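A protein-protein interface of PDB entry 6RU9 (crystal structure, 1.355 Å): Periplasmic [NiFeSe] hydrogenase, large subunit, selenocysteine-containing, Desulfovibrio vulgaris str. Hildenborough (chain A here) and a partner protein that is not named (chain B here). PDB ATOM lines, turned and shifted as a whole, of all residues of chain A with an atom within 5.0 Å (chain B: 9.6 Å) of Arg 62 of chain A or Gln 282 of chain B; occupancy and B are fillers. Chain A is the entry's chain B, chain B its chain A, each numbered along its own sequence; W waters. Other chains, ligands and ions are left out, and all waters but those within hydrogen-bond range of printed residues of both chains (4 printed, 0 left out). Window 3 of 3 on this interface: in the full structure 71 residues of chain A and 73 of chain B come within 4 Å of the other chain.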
ATOM      1  N   ASP A  60     -33.558 -11.161  30.574  1.00  0.00           N
ATOM      2  CA  ASP A  60     -32.459 -12.068  30.928  1.00  0.00           C
ATOM      3  C   ASP A  60     -31.334 -11.200  31.444  1.00  0.00           C
ATOM      4  O   ASP A  60     -30.908 -10.265  30.730  1.00  0.00           O
ATOM      5  CB  ASP A  60     -32.087 -12.834  29.657  1.00  0.00           C
ATOM      6  CG  ASP A  60     -30.939 -13.832  29.841  1.00  0.00           C
ATOM      7  OD1 ASP A  60     -30.030 -13.650  30.694  1.00  0.00           O
ATOM      8  OD2 ASP A  60     -30.924 -14.807  29.050  1.00  0.00           O
ATOM      9  N   PRO A  61     -30.856 -11.417  32.676  1.00  0.00           N
ATOM     10  CA  PRO A  61     -29.808 -10.530  33.212  1.00  0.00           C
ATOM     11  C   PRO A  61     -28.565 -10.448  32.348  1.00  0.00           C
ATOM     12  O   PRO A  61     -27.926  -9.399  32.334  1.00  0.00           O
ATOM     13  CB  PRO A  61     -29.490 -11.121  34.602  1.00  0.00           C
ATOM     14  CG  PRO A  61     -30.762 -11.870  34.963  1.00  0.00           C
ATOM     15  CD  PRO A  61     -31.250 -12.447  33.654  1.00  0.00           C
ATOM     16  N   ARG A  62     -28.215 -11.514  31.616  1.00  0.00           N
ATOM     17  CA  ARG A  62     -27.045 -11.463  30.733  1.00  0.00           C
ATOM     18  C   ARG A  62     -27.201 -10.424  29.622  1.00  0.00           C
ATOM     19  O   ARG A  62     -26.199  -9.921  29.110  1.00  0.00           O
ATOM     20  CB  ARG A  62     -26.779 -12.832  30.107  1.00  0.00           C
ATOM     21  CG  ARG A  62     -26.493 -13.952  31.125  1.00  0.00           C
ATOM     22  CD  ARG A  62     -26.448 -15.322  30.440  1.00  0.00           C
ATOM     23  NE  ARG A  62     -27.773 -15.686  30.002  1.00  0.00           N
ATOM     24  CZ  ARG A  62     -28.073 -16.822  29.393  1.00  0.00           C
ATOM     25  NH1 ARG A  62     -27.109 -17.712  29.139  1.00  0.00           N
ATOM     26  NH2 ARG A  62     -29.322 -17.048  29.034  1.00  0.00           N
ATOM     27  N   ASP A  63     -28.437 -10.087  29.244  1.00  0.00           N
ATOM     28  CA  ASP A  63     -28.626  -9.068  28.219  1.00  0.00           C
ATOM     29  C   ASP A  63     -28.151  -7.703  28.695  1.00  0.00           C
ATOM     30  O   ASP A  63     -27.886  -6.816  27.872  1.00  0.00           O
ATOM     31  CB  ASP A  63     -30.098  -8.926  27.840  1.00  0.00           C
ATOM     32  CG  ASP A  63     -30.612 -10.083  27.015  1.00  0.00           C
ATOM     33  OD1 ASP A  63     -29.834 -11.008  26.675  1.00  0.00           O
ATOM     34  OD2 ASP A  63     -31.821 -10.058  26.734  1.00  0.00           O
ATOM     35  N   ALA A  64     -28.071  -7.495  30.007  1.00  0.00           N
ATOM     36  CA  ALA A  64     -27.747  -6.154  30.503  1.00  0.00           C
ATOM     37  C   ALA A  64     -26.406  -5.662  29.954  1.00  0.00           C
ATOM     38  O   ALA A  64     -26.247  -4.467  29.680  1.00  0.00           O
ATOM     39  CB  ALA A  64     -27.753  -6.114  32.023  1.00  0.00           C
ATOM     40  N   SER A  65     -25.402  -6.551  29.847  1.00  0.00           N
ATOM     41  CA  SER A  65     -24.069  -6.087  29.466  1.00  0.00           C
ATOM     42  C   SER A  65     -23.987  -5.652  28.010  1.00  0.00           C
ATOM     43  O   SER A  65     -22.964  -5.077  27.611  1.00  0.00           O
ATOM     44  CB  SER A  65     -23.015  -7.123  29.790  1.00  0.00           C
ATOM     45  OG  SER A  65     -23.337  -8.395  29.267  1.00  0.00           O
ATOM     46  N   GLN A  66     -25.022  -5.923  27.214  1.00  0.00           N
ATOM     47  CA  GLN A  66     -25.222  -5.302  25.907  1.00  0.00           C
ATOM     48  C   GLN A  66     -26.127  -4.078  25.981  1.00  0.00           C
ATOM     49  O   GLN A  66     -25.755  -2.999  25.515  1.00  0.00           O
ATOM     50  CB  GLN A  66     -25.727  -6.309  24.885  1.00  0.00           C
ATOM     51  CG  GLN A  66     -24.683  -7.318  24.472  1.00  0.00           C
ATOM     52  CD  GLN A  66     -23.497  -6.667  23.822  1.00  0.00           C
ATOM     53  OE1 GLN A  66     -23.639  -5.871  22.878  1.00  0.00           O
ATOM     54  NE2 GLN A  66     -22.318  -6.941  24.356  1.00  0.00           N
ATOM     55  N   LEU A  87     -23.026  -8.517  37.396  1.00  0.00           N
ATOM     56  CA  LEU A  87     -23.459  -9.865  37.040  1.00  0.00           C
ATOM     57  C   LEU A  87     -22.544 -10.941  37.611  1.00  0.00           C
ATOM     58  O   LEU A  87     -23.022 -11.996  38.045  1.00  0.00           O
ATOM     59  CB  LEU A  87     -23.531  -9.990  35.515  1.00  0.00           C
ATOM     60  CG  LEU A  87     -24.580  -9.101  34.884  1.00  0.00           C
ATOM     61  CD1 LEU A  87     -24.415  -9.164  33.360  1.00  0.00           C
ATOM     62  CD2 LEU A  87     -25.997  -9.461  35.281  1.00  0.00           C
ATOM     63  N   PHE A  91     -24.199 -13.769  39.792  1.00  0.00           N
ATOM     64  CA  PHE A  91     -24.142 -15.125  39.261  1.00  0.00           C
ATOM     65  C   PHE A  91     -23.170 -16.012  40.040  1.00  0.00           C
ATOM     66  O   PHE A  91     -23.156 -17.224  39.819  1.00  0.00           O
ATOM     67  CB  PHE A  91     -23.683 -15.123  37.793  1.00  0.00           C
ATOM     68  CG  PHE A  91     -24.748 -14.719  36.788  1.00  0.00           C
ATOM     69  CD1 PHE A  91     -25.560 -13.621  36.985  1.00  0.00           C
ATOM     70  CD2 PHE A  91     -24.897 -15.434  35.597  1.00  0.00           C
ATOM     71  CE1 PHE A  91     -26.516 -13.232  36.033  1.00  0.00           C
ATOM     72  CE2 PHE A  91     -25.860 -15.057  34.671  1.00  0.00           C
ATOM     73  CZ  PHE A  91     -26.645 -13.932  34.891  1.00  0.00           C
ATOM     74  N   VAL A 188     -20.714 -11.677  31.500  1.00  0.00           N
ATOM     75  CA  VAL A 188     -20.599 -12.275  32.827  1.00  0.00           C
ATOM     76  C   VAL A 188     -19.668 -13.468  32.702  1.00  0.00           C
ATOM     77  O   VAL A 188     -19.787 -14.265  31.762  1.00  0.00           O
ATOM     78  CB  VAL A 188     -21.983 -12.664  33.387  1.00  0.00           C
ATOM     79  CG1 VAL A 188     -22.644 -13.776  32.525  1.00  0.00           C
ATOM     80  CG2 VAL A 188     -21.858 -13.090  34.860  1.00  0.00           C
ATOM     81  N   VAL A 405     -27.751 -18.639  34.840  1.00  0.00           N
ATOM     82  CA  VAL A 405     -28.522 -17.525  35.396  1.00  0.00           C
ATOM     83  C   VAL A 405     -29.088 -17.953  36.747  1.00  0.00           C
ATOM     84  O   VAL A 405     -29.819 -18.959  36.832  1.00  0.00           O
ATOM     85  CB  VAL A 405     -29.623 -17.094  34.401  1.00  0.00           C
ATOM     86  CG1 VAL A 405     -30.512 -16.003  35.003  1.00  0.00           C
ATOM     87  CG2 VAL A 405     -29.007 -16.679  33.087  1.00  0.00           C
ATOM     88  N   ALA B 224     -19.765 -24.440  22.959  1.00  0.00           N
ATOM     89  CA  ALA B 224     -20.444 -24.377  24.243  1.00  0.00           C
ATOM     90  C   ALA B 224     -19.875 -23.315  25.167  1.00  0.00           C
ATOM     91  O   ALA B 224     -20.476 -23.026  26.200  1.00  0.00           O
ATOM     92  CB  ALA B 224     -20.350 -25.737  24.951  1.00  0.00           C
ATOM     93  N   PHE B 226     -17.898 -19.294  24.847  1.00  0.00           N
ATOM     94  CA  PHE B 226     -17.552 -18.221  23.930  1.00  0.00           C
ATOM     95  C   PHE B 226     -16.150 -18.357  23.369  1.00  0.00           C
ATOM     96  O   PHE B 226     -15.888 -17.987  22.217  1.00  0.00           O
ATOM     97  CB  PHE B 226     -17.659 -16.881  24.626  1.00  0.00           C
ATOM     98  CG  PHE B 226     -19.067 -16.484  24.969  1.00  0.00           C
ATOM     99  CD1 PHE B 226     -19.976 -16.181  23.961  1.00  0.00           C
ATOM    100  CD2 PHE B 226     -19.483 -16.391  26.288  1.00  0.00           C
ATOM    101  CE1 PHE B 226     -21.255 -15.755  24.269  1.00  0.00           C
ATOM    102  CE2 PHE B 226     -20.775 -15.992  26.597  1.00  0.00           C
ATOM    103  CZ  PHE B 226     -21.658 -15.681  25.580  1.00  0.00           C
ATOM    104  N   ARG B 233     -21.659 -20.368  16.509  1.00  0.00           N
ATOM    105  CA  ARG B 233     -22.091 -19.613  17.673  1.00  0.00           C
ATOM    106  C   ARG B 233     -23.599 -19.627  17.919  1.00  0.00           C
ATOM    107  O   ARG B 233     -24.080 -18.945  18.843  1.00  0.00           O
ATOM    108  CB  ARG B 233     -21.605 -18.170  17.563  1.00  0.00           C
ATOM    109  CG  ARG B 233     -20.105 -18.000  17.786  1.00  0.00           C
ATOM    110  CD  ARG B 233     -19.228 -18.556  16.640  1.00  0.00           C
ATOM    111  NE  ARG B 233     -17.950 -17.847  16.657  1.00  0.00           N
ATOM    112  CZ  ARG B 233     -16.750 -18.325  16.299  1.00  0.00           C
ATOM    113  NH1 ARG B 233     -16.594 -19.569  15.847  1.00  0.00           N
ATOM    114  NH2 ARG B 233     -15.681 -17.547  16.413  1.00  0.00           N
ATOM    115  N   TYR B 234     -24.351 -20.408  17.144  1.00  0.00           N
ATOM    116  CA  TYR B 234     -25.808 -20.364  17.236  1.00  0.00           C
ATOM    117  C   TYR B 234     -26.306 -20.675  18.641  1.00  0.00           C
ATOM    118  O   TYR B 234     -27.183 -19.974  19.173  1.00  0.00           O
ATOM    119  CB  TYR B 234     -26.413 -21.329  16.234  1.00  0.00           C
ATOM    120  CG  TYR B 234     -27.928 -21.407  16.255  1.00  0.00           C
ATOM    121  CD1 TYR B 234     -28.703 -20.552  15.483  1.00  0.00           C
ATOM    122  CD2 TYR B 234     -28.587 -22.357  17.020  1.00  0.00           C
ATOM    123  CE1 TYR B 234     -30.093 -20.625  15.471  1.00  0.00           C
ATOM    124  CE2 TYR B 234     -29.983 -22.451  17.005  1.00  0.00           C
ATOM    125  CZ  TYR B 234     -30.716 -21.571  16.235  1.00  0.00           C
ATOM    126  OH  TYR B 234     -32.093 -21.623  16.216  1.00  0.00           O
ATOM    127  N   ASP B 235     -25.768 -21.724  19.268  1.00  0.00           N
ATOM    128  CA  ASP B 235     -26.276 -22.083  20.589  1.00  0.00           C
ATOM    129  C   ASP B 235     -25.926 -21.036  21.638  1.00  0.00           C
ATOM    130  O   ASP B 235     -26.619 -20.934  22.658  1.00  0.00           O
ATOM    131  CB  ASP B 235     -25.742 -23.437  21.024  1.00  0.00           C
ATOM    132  CG  ASP B 235     -26.409 -24.625  20.305  1.00  0.00           C
ATOM    133  OD1 ASP B 235     -27.390 -24.447  19.552  1.00  0.00           O
ATOM    134  OD2 ASP B 235     -25.923 -25.763  20.527  1.00  0.00           O
ATOM    135  N   LEU B 236     -24.858 -20.261  21.412  1.00  0.00           N
ATOM    136  CA  LEU B 236     -24.477 -19.147  22.272  1.00  0.00           C
ATOM    137  C   LEU B 236     -25.308 -17.897  22.026  1.00  0.00           C
ATOM    138  O   LEU B 236     -25.099 -16.890  22.730  1.00  0.00           O
ATOM    139  CB  LEU B 236     -23.001 -18.821  22.064  1.00  0.00           C
ATOM    140  CG  LEU B 236     -22.011 -19.913  22.490  1.00  0.00           C
ATOM    141  CD1 LEU B 236     -20.634 -19.608  21.949  1.00  0.00           C
ATOM    142  CD2 LEU B 236     -21.965 -20.033  23.995  1.00  0.00           C
ATOM    143  N   GLY B 237     -26.219 -17.928  21.048  1.00  0.00           N
ATOM    144  CA  GLY B 237     -27.120 -16.829  20.793  1.00  0.00           C
ATOM    145  C   GLY B 237     -26.963 -16.075  19.487  1.00  0.00           C
ATOM    146  O   GLY B 237     -27.673 -15.074  19.292  1.00  0.00           O
ATOM    147  N   CYS B 238     -26.083 -16.515  18.596  1.00  0.00           N
ATOM    148  CA  CYS B 238     -25.817 -15.765  17.364  1.00  0.00           C
ATOM    149  C   CYS B 238     -27.105 -15.557  16.570  1.00  0.00           C
ATOM    150  O   CYS B 238     -27.820 -16.520  16.279  1.00  0.00           O
ATOM    151  CB  CYS B 238     -24.822 -16.517  16.484  1.00  0.00           C
ATOM    152  SG  CYS B 238     -24.312 -15.528  15.062  1.00  0.00           S
ATOM    153  N   LYS B 239     -27.383 -14.296  16.199  1.00  0.00           N
ATOM    154  CA  LYS B 239     -28.558 -13.935  15.413  1.00  0.00           C
ATOM    155  C   LYS B 239     -28.232 -13.726  13.925  1.00  0.00           C
ATOM    156  O   LYS B 239     -29.034 -13.143  13.183  1.00  0.00           O
ATOM    157  CB  LYS B 239     -29.274 -12.733  16.023  1.00  0.00           C
ATOM    158  CG  LYS B 239     -29.626 -12.885  17.511  1.00  0.00           C
ATOM    159  CD  LYS B 239     -30.370 -14.183  17.788  1.00  0.00           C
ATOM    160  CE  LYS B 239     -30.968 -14.248  19.208  1.00  0.00           C
ATOM    161  NZ  LYS B 239     -29.948 -13.995  20.262  1.00  0.00           N
ATOM    162  N   GLY B 240     -27.053 -14.173  13.482  1.00  0.00           N
ATOM    163  CA  GLY B 240     -26.688 -14.062  12.087  1.00  0.00           C
ATOM    164  C   GLY B 240     -27.734 -14.559  11.115  1.00  0.00           C
ATOM    165  O   GLY B 240     -27.926 -13.943  10.048  1.00  0.00           O
ATOM    166  N   VAL B 264     -20.888 -13.150  19.545  1.00  0.00           N
ATOM    167  CA  VAL B 264     -22.052 -13.483  18.741  1.00  0.00           C
ATOM    168  C   VAL B 264     -22.546 -12.221  18.051  1.00  0.00           C
ATOM    169  O   VAL B 264     -22.333 -11.100  18.523  1.00  0.00           O
ATOM    170  CB  VAL B 264     -23.206 -14.080  19.594  1.00  0.00           C
ATOM    171  CG1 VAL B 264     -22.735 -15.336  20.317  1.00  0.00           C
ATOM    172  CG2 VAL B 264     -23.722 -13.063  20.567  1.00  0.00           C
ATOM    173  N   CYS B 265     -23.250 -12.409  16.934  1.00  0.00           N
ATOM    174  CA  CYS B 265     -24.036 -11.316  16.353  1.00  0.00           C
ATOM    175  C   CYS B 265     -25.315 -11.134  17.161  1.00  0.00           C
ATOM    176  O   CYS B 265     -26.017 -12.111  17.468  1.00  0.00           O
ATOM    177  CB  CYS B 265     -24.383 -11.632  14.899  1.00  0.00           C
ATOM    178  SG  CYS B 265     -25.451 -10.443  14.029  1.00  0.00           S
ATOM    179  N   ILE B 266     -25.648  -9.879  17.483  1.00  0.00           N
ATOM    180  CA  ILE B 266     -26.874  -9.534  18.213  1.00  0.00           C
ATOM    181  C   ILE B 266     -27.934  -8.907  17.309  1.00  0.00           C
ATOM    182  O   ILE B 266     -28.958  -8.407  17.808  1.00  0.00           O
ATOM    183  CB  ILE B 266     -26.595  -8.658  19.449  1.00  0.00           C
ATOM    184  CG1 ILE B 266     -26.081  -7.276  19.059  1.00  0.00           C
ATOM    185  CG2 ILE B 266     -25.599  -9.375  20.397  1.00  0.00           C
ATOM    186  CD1 ILE B 266     -25.906  -6.333  20.272  1.00  0.00           C
ATOM    187  N   ASP B 275     -35.596  -6.156  21.020  1.00  0.00           N
ATOM    188  CA  ASP B 275     -36.496  -7.123  21.651  1.00  0.00           C
ATOM    189  C   ASP B 275     -36.639  -8.407  20.833  1.00  0.00           C
ATOM    190  O   ASP B 275     -36.754  -9.491  21.409  1.00  0.00           O
ATOM    191  CB  ASP B 275     -37.855  -6.502  21.923  1.00  0.00           C
ATOM    192  CG  ASP B 275     -37.804  -5.461  23.020  1.00  0.00           C
ATOM    193  OD1 ASP B 275     -36.863  -5.477  23.861  1.00  0.00           O
ATOM    194  OD2 ASP B 275     -38.738  -4.655  23.051  1.00  0.00           O
ATOM    195  N   GLY B 276     -36.649  -8.324  19.503  1.00  0.00           N
ATOM    196  CA  GLY B 276     -36.762  -9.519  18.704  1.00  0.00           C
ATOM    197  C   GLY B 276     -35.482 -10.284  18.502  1.00  0.00           C
ATOM    198  O   GLY B 276     -35.457 -11.374  17.920  1.00  0.00           O
ATOM    199  N   LYS B 277     -34.386  -9.734  19.004  1.00  0.00           N
ATOM    200  CA  LYS B 277     -33.064 -10.348  18.956  1.00  0.00           C
ATOM    201  C   LYS B 277     -32.590 -10.818  20.326  1.00  0.00           C
ATOM    202  O   LYS B 277     -31.463 -11.315  20.446  1.00  0.00           O
ATOM    203  CB  LYS B 277     -32.076  -9.351  18.358  1.00  0.00           C
ATOM    204  CG  LYS B 277     -32.352  -9.036  16.890  1.00  0.00           C
ATOM    205  CD  LYS B 277     -32.055 -10.250  16.028  1.00  0.00           C
ATOM    206  CE  LYS B 277     -32.241  -9.983  14.520  1.00  0.00           C
ATOM    207  NZ  LYS B 277     -33.663  -9.831  14.158  1.00  0.00           N
ATOM    208  N   SER B 278     -33.426 -10.689  21.341  1.00  0.00           N
ATOM    209  CA  SER B 278     -33.136 -10.935  22.749  1.00  0.00           C
ATOM    210  C   SER B 278     -34.013 -12.080  23.228  1.00  0.00           C
ATOM    211  O   SER B 278     -35.143 -12.245  22.749  1.00  0.00           O
ATOM    212  CB  SER B 278     -33.550  -9.703  23.593  1.00  0.00           C
ATOM    213  OG  SER B 278     -32.747  -8.591  23.375  1.00  0.00           O
ATOM    214  N   PRO B 279     -33.562 -12.874  24.214  1.00  0.00           N
ATOM    215  CA  PRO B 279     -32.253 -12.878  24.870  1.00  0.00           C
ATOM    216  C   PRO B 279     -31.081 -13.082  23.941  1.00  0.00           C
ATOM    217  O   PRO B 279     -31.110 -13.885  23.001  1.00  0.00           O
ATOM    218  CB  PRO B 279     -32.329 -14.070  25.858  1.00  0.00           C
ATOM    219  CG  PRO B 279     -33.681 -14.666  25.671  1.00  0.00           C
ATOM    220  CD  PRO B 279     -34.546 -13.701  24.941  1.00  0.00           C
ATOM    221  N   PHE B 280     -30.034 -12.300  24.190  1.00  0.00           N
ATOM    222  CA  PHE B 280     -28.906 -12.268  23.273  1.00  0.00           C
ATOM    223  C   PHE B 280     -28.094 -13.558  23.316  1.00  0.00           C
ATOM    224  O   PHE B 280     -27.468 -13.914  22.308  1.00  0.00           O
ATOM    225  CB  PHE B 280     -28.010 -11.077  23.598  1.00  0.00           C
ATOM    226  CG  PHE B 280     -28.626  -9.773  23.264  1.00  0.00           C
ATOM    227  CD1 PHE B 280     -29.111  -9.540  21.992  1.00  0.00           C
ATOM    228  CD2 PHE B 280     -28.718  -8.770  24.203  1.00  0.00           C
ATOM    229  CE1 PHE B 280     -29.681  -8.308  21.662  1.00  0.00           C
ATOM    230  CE2 PHE B 280     -29.312  -7.527  23.875  1.00  0.00           C
ATOM    231  CZ  PHE B 280     -29.774  -7.308  22.626  1.00  0.00           C
ATOM    232  N   TYR B 281     -28.064 -14.249  24.458  1.00  0.00           N
ATOM    233  CA  TYR B 281     -27.152 -15.362  24.674  1.00  0.00           C
ATOM    234  C   TYR B 281     -27.867 -16.707  24.708  1.00  0.00           C
ATOM    235  O   TYR B 281     -27.352 -17.673  25.287  1.00  0.00           O
ATOM    236  CB  TYR B 281     -26.282 -15.112  25.900  1.00  0.00           C
ATOM    237  CG  TYR B 281     -25.454 -13.855  25.674  1.00  0.00           C
ATOM    238  CD1 TYR B 281     -24.495 -13.795  24.671  1.00  0.00           C
ATOM    239  CD2 TYR B 281     -25.694 -12.703  26.410  1.00  0.00           C
ATOM    240  CE1 TYR B 281     -23.745 -12.633  24.439  1.00  0.00           C
ATOM    241  CE2 TYR B 281     -24.953 -11.540  26.180  1.00  0.00           C
ATOM    242  CZ  TYR B 281     -23.977 -11.520  25.220  1.00  0.00           C
ATOM    243  OH  TYR B 281     -23.257 -10.381  25.001  1.00  0.00           O
ATOM    244  N   GLN B 282     -29.022 -16.785  24.070  1.00  0.00           N
ATOM    245  CA  GLN B 282     -29.626 -18.054  23.691  1.00  0.00           C
ATOM    246  C   GLN B 282     -30.326 -17.864  22.355  1.00  0.00           C
ATOM    247  O   GLN B 282     -30.572 -16.742  21.896  1.00  0.00           O
ATOM    248  CB  GLN B 282     -30.520 -18.613  24.795  1.00  0.00           C
ATOM    249  CG  GLN B 282     -31.713 -17.799  25.076  1.00  0.00           C
ATOM    250  CD  GLN B 282     -32.347 -18.154  26.409  1.00  0.00           C
ATOM    251  OE1 GLN B 282     -31.683 -18.679  27.310  1.00  0.00           O
ATOM    252  NE2 GLN B 282     -33.640 -17.874  26.548  1.00  0.00           N
ATOM    253  N   ALA B 283     -30.609 -18.992  21.697  1.00  0.00           N
ATOM    254  CA  ALA B 283     -31.144 -18.939  20.346  1.00  0.00           C
ATOM    255  C   ALA B 283     -32.473 -18.188  20.225  1.00  0.00           C
ATOM    256  O   ALA B 283     -32.778 -17.579  19.181  1.00  0.00           O
ATOM    257  CB  ALA B 283     -31.273 -20.368  19.790  1.00  0.00           C
ATOM    258  OXT ALA B 283     -33.278 -18.126  21.148  1.00  0.00           O
HETATM  259  O   HOH W   1     -29.061 -13.612  27.173  1.00  0.00           O
HETATM  260  O   HOH W   2     -33.196 -16.350  29.025  1.00  0.00           O
HETATM  261  O   HOH W   3     -22.152  -8.719  26.853  1.00  0.00           O
HETATM  262  O   HOH W   4     -32.636  -7.620  25.831  1.00  0.00           O
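OD1 of Asp 63 of chain A is in hydrogen-bond range of N of Phe 280 of chain B, at 2.8 Å.
The guanidinium group (NH2) of Arg 62 of chain A is in hydrogen-bond range of the side-chain amide oxygen (OE1) of Gln 282 of chain B.
O of Pro 279 of chain B sits at hydrogen-bond distance from NZ of Lys 239 of chain B, at 3.0 Å.
The side-chain amino group (NZ) of Lys 239 of chain B lies within hydrogen-bond range of the backbone carbonyl oxygen (O) of Phe 280 of chain B, 3.2 Å away.
The side-chain amino group of Lys 239 of chain B sits at hydrogen-bond distance from the backbone carbonyl oxygen of Gln 282 of chain B.
OD2 of Asp 60 of chain A is in salt-bridge range of NH2 of Arg 62 of chain A (2.8 Å).
The backbone carbonyl oxygen (O) of Arg 62 of chain A lies within hydrogen-bond range of the side-chain hydroxyl (OG) of Ser 65 of chain A.
Among the printed residues, merely in contact across the chains: Asp 63 of chain A with Pro 279 of chain B (3.4 Å), Gln 66 of chain A with Tyr 281 of chain B (3.4 Å), Gln 66 of chain A with Ile 266 of chain B (3.5 Å), Asp 60 of chain A with Pro 279 of chain B (3.6 Å), Arg 62 of chain A with Tyr 281 of chain B (3.6 Å), Asp 63 of chain A with Ser 278 of chain B (3.6 Å) and Gln 66 of chain A with Phe 280 of chain B (3.9 Å).
Of the printed residues of chain B, Asp 60 of chain A touches Pro 279.
No residue of chain B comes within 4 Å of Pro 61 of chain A.
Of chain B, only Tyr 281 (3.6 Å) and Gln 282 (3.3 Å) come within 4 Å of Arg 62 of chain A.
Of the printed residues of chain B, Asp 63 of chain A touches Ser 278 (3.6 Å), Pro 279 (3.4 Å) and Phe 280 (2.8 Å).
No residue of chain B comes within 4 Å of Ala 64 of chain A.
Phe 91 of chain A touches none of the printed residues of chain B.
Of the printed residues of chain A, Ile 266 of chain B touches Gln 66 (3.5 Å).
Of the printed residues of chain A, Ser 278 of chain B touches Asp 63 (3.6 Å).
Printed residues of chain A within 4 Å of Pro 279 of chain B: Asp 60 and Asp 63.
Of the printed residues of chain A, Phe 280 of chain B touches Asp 63 (2.8 Å) and Gln 66 (3.9 Å).
Of the printed residues of chain A, Tyr 281 of chain B touches Arg 62 (3.6 Å) and Gln 66 (3.4 Å).
Of the printed residues of chain A, Gln 282 of chain B touches Arg 62.
The nearest residue of chain B that does not touch Arg 62 of chain A is Pro 279 of chain B (5.3 Å).
Of the 11 printed residues of chain A, 4 touch a printed residue of chain B.
Printed residues of chain A that touch a printed residue of chain B: Asp 60, Arg 62, Asp 63 and Gln 66.
Along chain A the printed residues that touch a printed residue of chain B span positions 60 to 66.
Hydrophobic or aromatic side chains of chain B that line the printed part of chain A: Ile 266, Pro 279, Phe 280 and Tyr 281.
Among the printed residues, no Asp or Glu carboxylate lies within 4 Å of a Lys or Arg side-chain nitrogen of the other chain.
Water W4 lies within hydrogen-bond range of OG of Ser 278 of chain B (2.6 Å) and OD2 of Asp 63 of chain A (2.7 Å).
Water W3 lies within hydrogen-bond range of OG of Ser 65 of chain A (2.7 Å), OH of Tyr 281 of chain B (2.7 Å) and NE2 of Gln 66 of chain A (3.1 Å).
Water W2 bridges OD2 of Asp 60 of chain A (2.7 Å) and NE2 of Gln 282 of chain B (2.9 Å).
Water W1 lies within hydrogen-bond range of the side-chain carboxylate (OD1) of Asp 63 of chain A (2.8 Å), the side-chain carboxylate (OD2) of Asp 60 of chain A (2.9 Å), the backbone NH (N) of Tyr 281 of chain B (3.0 Å) and the backbone NH (N) of Phe 280 of chain B (3.4 Å).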
